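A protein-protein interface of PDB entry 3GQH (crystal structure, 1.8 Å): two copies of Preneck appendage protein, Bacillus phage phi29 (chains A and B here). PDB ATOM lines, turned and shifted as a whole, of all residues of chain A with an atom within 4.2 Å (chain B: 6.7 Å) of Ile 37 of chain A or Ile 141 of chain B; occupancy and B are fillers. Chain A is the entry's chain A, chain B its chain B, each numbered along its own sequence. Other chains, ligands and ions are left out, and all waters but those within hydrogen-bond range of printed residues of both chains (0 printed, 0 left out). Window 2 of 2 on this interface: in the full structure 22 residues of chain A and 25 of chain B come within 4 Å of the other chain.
The backbone carbonyl oxygen of Ile 37 of chain A lies within hydrogen-bond range of the side-chain amino group of Lys 163 of chain B, 2.8 Å away.
O of Leu 109 of chain A sits at hydrogen-bond distance from NZ of Lys 163 of chain B (2.9 Å).
N of Ile 37 of chain A is in hydrogen-bond range of O of Val 20 of chain A, at 2.9 Å.
The side-chain amide nitrogen (NE2) of Gln 123 of chain B sits at hydrogen-bond distance from the backbone carbonyl oxygen (O) of Gln 143 of chain B, at 2.8 Å.
O of Phe 140 of chain B lies within hydrogen-bond range of OG of Ser 126 of chain B (2.5 Å).
The backbone carbonyl oxygen (O) of Ile 141 of chain B is in hydrogen-bond range of the backbone NH (N) of Leu 161 of chain B.
O of Ile 159 of chain B lies within hydrogen-bond range of N of Gln 143 of chain B.
Among the printed residues, merely in contact across the chains: Phe 6 of chain A with Gln 143 of chain B, Phe 6 of chain A with Leu 161 of chain B, Leu 22 of chain A with Gln 143 of chain B, Leu 22 of chain A with Leu 161 of chain B, Lys 35 of chain A with Phe 140 of chain B, Lys 35 of chain A with Ile 141 of chain B, Ile 37 of chain A with Ile 141 of chain B and Ile 37 of chain A with Leu 161 of chain B.
Of chain B, only Ile 141 (3.7 Å), Leu 161 (3.6 Å) and Lys 163 (2.8 Å) come within 4 Å of Ile 37 of chain A.
Of chain A, only Lys 35 (3.7 Å) and Ile 37 (3.7 Å) come within 4 Å of Ile 141 of chain B.
Of the printed residues of chain B, Phe 6 of chain A touches Gln 143 (3.6 Å) and Leu 161 (3.9 Å).
Of the printed residues of chain A, Leu 161 of chain B touches Phe 6, Leu 22 and Ile 37.
Of the printed residues of chain B, Leu 22 of chain A touches Gln 143 and Leu 161.
Val 162 of chain B touches none of the printed residues of chain A.
The nearest printed residue of chain B that does not touch Leu 22 of chain A is Ile 141 of chain B (4.1 Å).
Of the 9 printed residues of chain A, 5 touch a printed residue of chain B.
Printed residues of chain A that touch a printed residue of chain B: Phe 6, Leu 22, Lys 35, Ile 37 and Leu 109.
Hydrophobic or aromatic side chains of chain A that line the printed part of chain B: Phe 6, Leu 22 and Ile 37.
Printed residues of chain B that touch a printed residue of chain A: Phe 140, Ile 141, Gln 143, Leu 161 and Lys 163.
Hydrophobic or aromatic side chains of chain B within 4 Å of the printed part of chain A: Ile 141 and Leu 161.
No position is printed for both chains.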
ATOM      1  N   PHE A   6      17.129  -1.688  19.289  1.00  0.00           N
ATOM      2  CA  PHE A   6      18.477  -1.845  19.846  1.00  0.00           C
ATOM      3  C   PHE A   6      19.452  -1.049  18.988  1.00  0.00           C
ATOM      4  O   PHE A   6      19.229  -0.885  17.802  1.00  0.00           O
ATOM      5  CB  PHE A   6      18.936  -3.286  19.761  1.00  0.00           C
ATOM      6  CG  PHE A   6      18.155  -4.246  20.630  1.00  0.00           C
ATOM      7  CD1 PHE A   6      16.936  -4.770  20.189  1.00  0.00           C
ATOM      8  CD2 PHE A   6      18.675  -4.645  21.848  1.00  0.00           C
ATOM      9  CE1 PHE A   6      16.228  -5.689  20.972  1.00  0.00           C
ATOM     10  CE2 PHE A   6      17.990  -5.555  22.641  1.00  0.00           C
ATOM     11  CZ  PHE A   6      16.755  -6.070  22.204  1.00  0.00           C
ATOM     12  N   VAL A  20      21.366 -11.432  15.142  1.00  0.00           N
ATOM     13  CA  VAL A  20      22.192 -10.567  15.989  1.00  0.00           C
ATOM     14  C   VAL A  20      22.350 -11.082  17.428  1.00  0.00           C
ATOM     15  O   VAL A  20      21.520 -11.845  17.930  1.00  0.00           O
ATOM     16  CB  VAL A  20      21.709  -9.085  15.984  1.00  0.00           C
ATOM     17  CG1 VAL A  20      21.851  -8.483  14.584  1.00  0.00           C
ATOM     18  CG2 VAL A  20      20.256  -8.948  16.499  1.00  0.00           C
ATOM     19  N   LEU A  22      24.180  -9.616  21.478  1.00  0.00           N
ATOM     20  CA  LEU A  22      24.539  -8.421  22.235  1.00  0.00           C
ATOM     21  C   LEU A  22      26.008  -8.462  22.646  1.00  0.00           C
ATOM     22  O   LEU A  22      26.514  -9.500  23.070  1.00  0.00           O
ATOM     23  CB  LEU A  22      23.681  -8.313  23.501  1.00  0.00           C
ATOM     24  CG  LEU A  22      22.216  -7.922  23.306  1.00  0.00           C
ATOM     25  CD1 LEU A  22      21.462  -8.174  24.594  1.00  0.00           C
ATOM     26  CD2 LEU A  22      22.100  -6.449  22.891  1.00  0.00           C
ATOM     27  N   ILE A  27      24.037  -4.179  19.590  1.00  0.00           N
ATOM     28  CA  ILE A  27      23.938  -5.363  18.724  1.00  0.00           C
ATOM     29  C   ILE A  27      25.027  -5.461  17.651  1.00  0.00           C
ATOM     30  O   ILE A  27      25.551  -4.441  17.147  1.00  0.00           O
ATOM     31  CB  ILE A  27      22.509  -5.558  18.111  1.00  0.00           C
ATOM     32  CG1 ILE A  27      22.096  -4.331  17.307  1.00  0.00           C
ATOM     33  CG2 ILE A  27      21.458  -5.874  19.227  1.00  0.00           C
ATOM     34  CD1 ILE A  27      20.990  -4.570  16.318  1.00  0.00           C
ATOM     35  N   LYS A  35      24.766 -16.388  21.904  1.00  0.00           N
ATOM     36  CA  LYS A  35      23.329 -16.299  22.130  1.00  0.00           C
ATOM     37  C   LYS A  35      22.713 -15.444  21.032  1.00  0.00           C
ATOM     38  O   LYS A  35      23.023 -14.259  20.916  1.00  0.00           O
ATOM     39  CB  LYS A  35      23.040 -15.653  23.482  1.00  0.00           C
ATOM     40  CG  LYS A  35      23.689 -16.343  24.680  1.00  0.00           C
ATOM     41  CD  LYS A  35      23.002 -15.949  25.987  1.00  0.00           C
ATOM     42  CE  LYS A  35      21.570 -16.508  26.032  1.00  0.00           C
ATOM     43  NZ  LYS A  35      21.047 -16.710  27.408  1.00  0.00           N
ATOM     44  N   ILE A  36      21.849 -16.038  20.219  1.00  0.00           N
ATOM     45  CA  ILE A  36      21.141 -15.279  19.180  1.00  0.00           C
ATOM     46  C   ILE A  36      19.901 -14.636  19.815  1.00  0.00           C
ATOM     47  O   ILE A  36      18.999 -15.341  20.272  1.00  0.00           O
ATOM     48  CB  ILE A  36      20.730 -16.192  17.987  1.00  0.00           C
ATOM     49  CG1 ILE A  36      21.965 -16.838  17.342  1.00  0.00           C
ATOM     50  CG2 ILE A  36      19.880 -15.404  16.969  1.00  0.00           C
ATOM     51  CD1 ILE A  36      21.643 -18.024  16.436  1.00  0.00           C
ATOM     52  N   ILE A  37      19.851 -13.313  19.838  1.00  0.00           N
ATOM     53  CA  ILE A  37      18.760 -12.604  20.510  1.00  0.00           C
ATOM     54  C   ILE A  37      17.584 -12.336  19.587  1.00  0.00           C
ATOM     55  O   ILE A  37      16.432 -12.183  20.030  1.00  0.00           O
ATOM     56  CB  ILE A  37      19.221 -11.296  21.190  1.00  0.00           C
ATOM     57  CG1 ILE A  37      19.556 -10.211  20.148  1.00  0.00           C
ATOM     58  CG2 ILE A  37      20.395 -11.562  22.148  1.00  0.00           C
ATOM     59  CD1 ILE A  37      19.328  -8.799  20.638  1.00  0.00           C
ATOM     60  N   GLY A  38      17.853 -12.326  18.289  1.00  0.00           N
ATOM     61  CA  GLY A  38      16.809 -12.018  17.335  1.00  0.00           C
ATOM     62  C   GLY A  38      17.382 -11.681  15.973  1.00  0.00           C
ATOM     63  O   GLY A  38      18.550 -12.000  15.693  1.00  0.00           O
ATOM     64  N   LEU A 109      12.128 -10.312  18.103  1.00  0.00           N
ATOM     65  CA  LEU A 109      12.545 -11.113  19.252  1.00  0.00           C
ATOM     66  C   LEU A 109      11.680 -12.364  19.366  1.00  0.00           C
ATOM     67  O   LEU A 109      12.093 -13.359  19.979  1.00  0.00           O
ATOM     68  CB  LEU A 109      12.353 -10.313  20.545  1.00  0.00           C
ATOM     69  CG  LEU A 109      13.210  -9.057  20.711  1.00  0.00           C
ATOM     70  CD1 LEU A 109      12.831  -8.367  22.027  1.00  0.00           C
ATOM     71  CD2 LEU A 109      14.665  -9.449  20.709  1.00  0.00           C
ATOM     72  N   LYS B 122      27.524  -8.608  36.230  1.00  0.00           N
ATOM     73  CA  LYS B 122      28.439  -8.031  35.238  1.00  0.00           C
ATOM     74  C   LYS B 122      27.782  -7.873  33.874  1.00  0.00           C
ATOM     75  O   LYS B 122      27.070  -8.762  33.408  1.00  0.00           O
ATOM     76  CB  LYS B 122      29.669  -8.929  35.084  1.00  0.00           C
ATOM     77  CG  LYS B 122      30.533  -9.068  36.341  1.00  0.00           C
ATOM     78  CD  LYS B 122      31.499 -10.258  36.210  1.00  0.00           C
ATOM     79  CE  LYS B 122      30.778 -11.604  36.388  1.00  0.00           C
ATOM     80  NZ  LYS B 122      31.709 -12.760  36.301  1.00  0.00           N
ATOM     81  N   GLN B 123      28.050  -6.746  33.219  1.00  0.00           N
ATOM     82  CA  GLN B 123      27.648  -6.567  31.827  1.00  0.00           C
ATOM     83  C   GLN B 123      28.114  -7.740  30.973  1.00  0.00           C
ATOM     84  O   GLN B 123      29.258  -8.200  31.093  1.00  0.00           O
ATOM     85  CB  GLN B 123      28.207  -5.251  31.273  1.00  0.00           C
ATOM     86  CG  GLN B 123      27.826  -4.977  29.835  1.00  0.00           C
ATOM     87  CD  GLN B 123      28.382  -3.664  29.336  1.00  0.00           C
ATOM     88  OE1 GLN B 123      29.561  -3.370  29.535  1.00  0.00           O
ATOM     89  NE2 GLN B 123      27.541  -2.864  28.688  1.00  0.00           N
ATOM     90  N   GLY B 124      27.218  -8.238  30.127  1.00  0.00           N
ATOM     91  CA  GLY B 124      27.529  -9.304  29.186  1.00  0.00           C
ATOM     92  C   GLY B 124      27.545 -10.709  29.766  1.00  0.00           C
ATOM     93  O   GLY B 124      27.939 -11.660  29.099  1.00  0.00           O
ATOM     94  N   HIS B 125      27.111 -10.842  31.011  1.00  0.00           N
ATOM     95  CA  HIS B 125      26.942 -12.140  31.620  1.00  0.00           C
ATOM     96  C   HIS B 125      25.476 -12.387  31.949  1.00  0.00           C
ATOM     97  O   HIS B 125      24.640 -11.509  31.777  1.00  0.00           O
ATOM     98  CB  HIS B 125      27.801 -12.235  32.872  1.00  0.00           C
ATOM     99  CG  HIS B 125      29.270 -12.263  32.579  1.00  0.00           C
ATOM    100  ND1 HIS B 125      30.021 -13.418  32.659  1.00  0.00           N
ATOM    101  CD2 HIS B 125      30.118 -11.287  32.175  1.00  0.00           C
ATOM    102  CE1 HIS B 125      31.274 -13.145  32.340  1.00  0.00           C
ATOM    103  NE2 HIS B 125      31.361 -11.860  32.042  1.00  0.00           N
ATOM    104  N   SER B 126      25.174 -13.585  32.433  1.00  0.00           N
ATOM    105  CA  SER B 126      23.811 -13.902  32.809  1.00  0.00           C
ATOM    106  C   SER B 126      23.561 -13.679  34.302  1.00  0.00           C
ATOM    107  O   SER B 126      24.441 -13.225  35.036  1.00  0.00           O
ATOM    108  CB  SER B 126      23.507 -15.345  32.435  1.00  0.00           C
ATOM    109  OG  SER B 126      23.484 -15.542  31.024  1.00  0.00           O
ATOM    110  N   ILE B 127      22.345 -13.994  34.752  1.00  0.00           N
ATOM    111  CA  ILE B 127      21.968 -13.763  36.153  1.00  0.00           C
ATOM    112  C   ILE B 127      21.210 -14.959  36.733  1.00  0.00           C
ATOM    113  O   ILE B 127      20.672 -15.771  35.979  1.00  0.00           O
ATOM    114  CB  ILE B 127      21.121 -12.466  36.318  1.00  0.00           C
ATOM    115  CG1 ILE B 127      19.818 -12.530  35.488  1.00  0.00           C
ATOM    116  CG2 ILE B 127      21.941 -11.234  35.940  1.00  0.00           C
ATOM    117  CD1 ILE B 127      18.773 -11.399  35.813  1.00  0.00           C
ATOM    118  N   ASN B 139      21.093 -17.160  33.447  1.00  0.00           N
ATOM    119  CA  ASN B 139      19.878 -16.728  32.751  1.00  0.00           C
ATOM    120  C   ASN B 139      20.051 -15.380  32.068  1.00  0.00           C
ATOM    121  O   ASN B 139      20.608 -14.459  32.652  1.00  0.00           O
ATOM    122  CB  ASN B 139      18.697 -16.560  33.715  1.00  0.00           C
ATOM    123  CG  ASN B 139      18.287 -17.848  34.380  1.00  0.00           C
ATOM    124  OD1 ASN B 139      17.546 -18.645  33.803  1.00  0.00           O
ATOM    125  ND2 ASN B 139      18.762 -18.058  35.604  1.00  0.00           N
ATOM    126  N   PHE B 140      19.537 -15.262  30.845  1.00  0.00           N
ATOM    127  CA  PHE B 140      19.402 -13.957  30.177  1.00  0.00           C
ATOM    128  C   PHE B 140      20.751 -13.313  29.848  1.00  0.00           C
ATOM    129  O   PHE B 140      21.806 -13.967  29.931  1.00  0.00           O
ATOM    130  CB  PHE B 140      18.536 -12.989  31.010  1.00  0.00           C
ATOM    131  CG  PHE B 140      17.295 -13.618  31.634  1.00  0.00           C
ATOM    132  CD1 PHE B 140      17.023 -13.425  32.992  1.00  0.00           C
ATOM    133  CD2 PHE B 140      16.405 -14.375  30.874  1.00  0.00           C
ATOM    134  CE1 PHE B 140      15.883 -13.974  33.586  1.00  0.00           C
ATOM    135  CE2 PHE B 140      15.246 -14.924  31.460  1.00  0.00           C
ATOM    136  CZ  PHE B 140      14.995 -14.728  32.816  1.00  0.00           C
ATOM    137  N   ILE B 141      20.722 -12.041  29.458  1.00  0.00           N
ATOM    138  CA  ILE B 141      21.948 -11.293  29.186  1.00  0.00           C
ATOM    139  C   ILE B 141      21.884  -9.906  29.817  1.00  0.00           C
ATOM    140  O   ILE B 141      20.926  -9.166  29.591  1.00  0.00           O
ATOM    141  CB  ILE B 141      22.165 -11.094  27.649  1.00  0.00           C
ATOM    142  CG1 ILE B 141      22.099 -12.432  26.904  1.00  0.00           C
ATOM    143  CG2 ILE B 141      23.493 -10.374  27.392  1.00  0.00           C
ATOM    144  CD1 ILE B 141      22.051 -12.302  25.363  1.00  0.00           C
ATOM    145  N   VAL B 142      22.896  -9.551  30.601  1.00  0.00           N
ATOM    146  CA  VAL B 142      22.990  -8.196  31.127  1.00  0.00           C
ATOM    147  C   VAL B 142      23.482  -7.250  30.022  1.00  0.00           C
ATOM    148  O   VAL B 142      24.598  -7.416  29.512  1.00  0.00           O
ATOM    149  CB  VAL B 142      23.894  -8.102  32.379  1.00  0.00           C
ATOM    150  CG1 VAL B 142      23.968  -6.662  32.861  1.00  0.00           C
ATOM    151  CG2 VAL B 142      23.353  -8.975  33.494  1.00  0.00           C
ATOM    152  N   GLN B 143      22.644  -6.275  29.663  1.00  0.00           N
ATOM    153  CA  GLN B 143      22.969  -5.317  28.602  1.00  0.00           C
ATOM    154  C   GLN B 143      23.887  -4.222  29.094  1.00  0.00           C
ATOM    155  O   GLN B 143      24.928  -3.955  28.496  1.00  0.00           O
ATOM    156  CB  GLN B 143      21.709  -4.678  28.030  1.00  0.00           C
ATOM    157  CG  GLN B 143      21.020  -5.529  27.031  1.00  0.00           C
ATOM    158  CD  GLN B 143      19.872  -4.821  26.347  1.00  0.00           C
ATOM    159  OE1 GLN B 143      19.931  -3.628  26.016  1.00  0.00           O
ATOM    160  NE2 GLN B 143      18.826  -5.555  26.122  1.00  0.00           N
ATOM    161  N   GLU B 144      23.492  -3.564  30.176  1.00  0.00           N
ATOM    162  CA  GLU B 144      24.339  -2.546  30.777  1.00  0.00           C
ATOM    163  C   GLU B 144      23.869  -2.222  32.169  1.00  0.00           C
ATOM    164  O   GLU B 144      22.679  -2.330  32.462  1.00  0.00           O
ATOM    165  CB  GLU B 144      24.400  -1.272  29.925  1.00  0.00           C
ATOM    166  CG  GLU B 144      23.101  -0.538  29.743  1.00  0.00           C
ATOM    167  CD  GLU B 144      23.306   0.770  28.996  1.00  0.00           C
ATOM    168  OE1 GLU B 144      23.943   1.690  29.556  1.00  0.00           O
ATOM    169  OE2 GLU B 144      22.845   0.859  27.838  1.00  0.00           O
ATOM    170  N   ILE B 159      19.966  -3.052  32.834  1.00  0.00           N
ATOM    171  CA  ILE B 159      19.024  -3.434  31.797  1.00  0.00           C
ATOM    172  C   ILE B 159      19.408  -4.835  31.388  1.00  0.00           C
ATOM    173  O   ILE B 159      20.572  -5.084  31.072  1.00  0.00           O
ATOM    174  CB  ILE B 159      19.104  -2.518  30.561  1.00  0.00           C
ATOM    175  CG1 ILE B 159      18.857  -1.042  30.945  1.00  0.00           C
ATOM    176  CG2 ILE B 159      18.142  -3.006  29.488  1.00  0.00           C
ATOM    177  CD1 ILE B 159      17.595  -0.803  31.763  1.00  0.00           C
ATOM    178  N   VAL B 160      18.431  -5.741  31.428  1.00  0.00           N
ATOM    179  CA  VAL B 160      18.631  -7.163  31.132  1.00  0.00           C
ATOM    180  C   VAL B 160      17.699  -7.517  29.968  1.00  0.00           C
ATOM    181  O   VAL B 160      16.550  -7.073  29.927  1.00  0.00           O
ATOM    182  CB  VAL B 160      18.332  -8.025  32.383  1.00  0.00           C
ATOM    183  CG1 VAL B 160      18.365  -9.524  32.085  1.00  0.00           C
ATOM    184  CG2 VAL B 160      19.346  -7.711  33.503  1.00  0.00           C
ATOM    185  N   LEU B 161      18.194  -8.290  29.004  1.00  0.00           N
ATOM    186  CA  LEU B 161      17.326  -8.760  27.925  1.00  0.00           C
ATOM    187  C   LEU B 161      16.744 -10.063  28.437  1.00  0.00           C
ATOM    188  O   LEU B 161      17.466 -11.044  28.593  1.00  0.00           O
ATOM    189  CB  LEU B 161      18.094  -8.980  26.607  1.00  0.00           C
ATOM    190  CG  LEU B 161      17.190  -9.518  25.481  1.00  0.00           C
ATOM    191  CD1 LEU B 161      16.058  -8.562  25.181  1.00  0.00           C
ATOM    192  CD2 LEU B 161      17.970  -9.816  24.204  1.00  0.00           C
ATOM    193  N   VAL B 162      15.453 -10.015  28.761  1.00  0.00           N
ATOM    194  CA  VAL B 162      14.676 -11.159  29.249  1.00  0.00           C
ATOM    195  C   VAL B 162      13.941 -11.835  28.093  1.00  0.00           C
ATOM    196  O   VAL B 162      13.289 -11.176  27.284  1.00  0.00           O
ATOM    197  CB  VAL B 162      13.657 -10.701  30.310  1.00  0.00           C
ATOM    198  CG1 VAL B 162      12.773 -11.871  30.764  1.00  0.00           C
ATOM    199  CG2 VAL B 162      14.364 -10.093  31.499  1.00  0.00           C
ATOM    200  N   LYS B 163      14.072 -13.158  28.009  1.00  0.00           N
ATOM    201  CA  LYS B 163      13.330 -13.976  27.033  1.00  0.00           C
ATOM    202  C   LYS B 163      12.934 -15.306  27.695  1.00  0.00           C
ATOM    203  O   LYS B 163      13.743 -15.918  28.401  1.00  0.00           O
ATOM    204  CB  LYS B 163      14.175 -14.253  25.775  1.00  0.00           C
ATOM    205  CG  LYS B 163      14.611 -13.019  24.964  1.00  0.00           C
ATOM    206  CD  LYS B 163      15.210 -13.388  23.590  1.00  0.00           C
ATOM    207  CE  LYS B 163      14.107 -13.696  22.564  1.00  0.00           C
ATOM    208  NZ  LYS B 163      14.640 -13.942  21.186  1.00  0.00           N
ATOM    209  OXT LYS B 163      11.807 -15.802  27.560  1.00  0.00           O
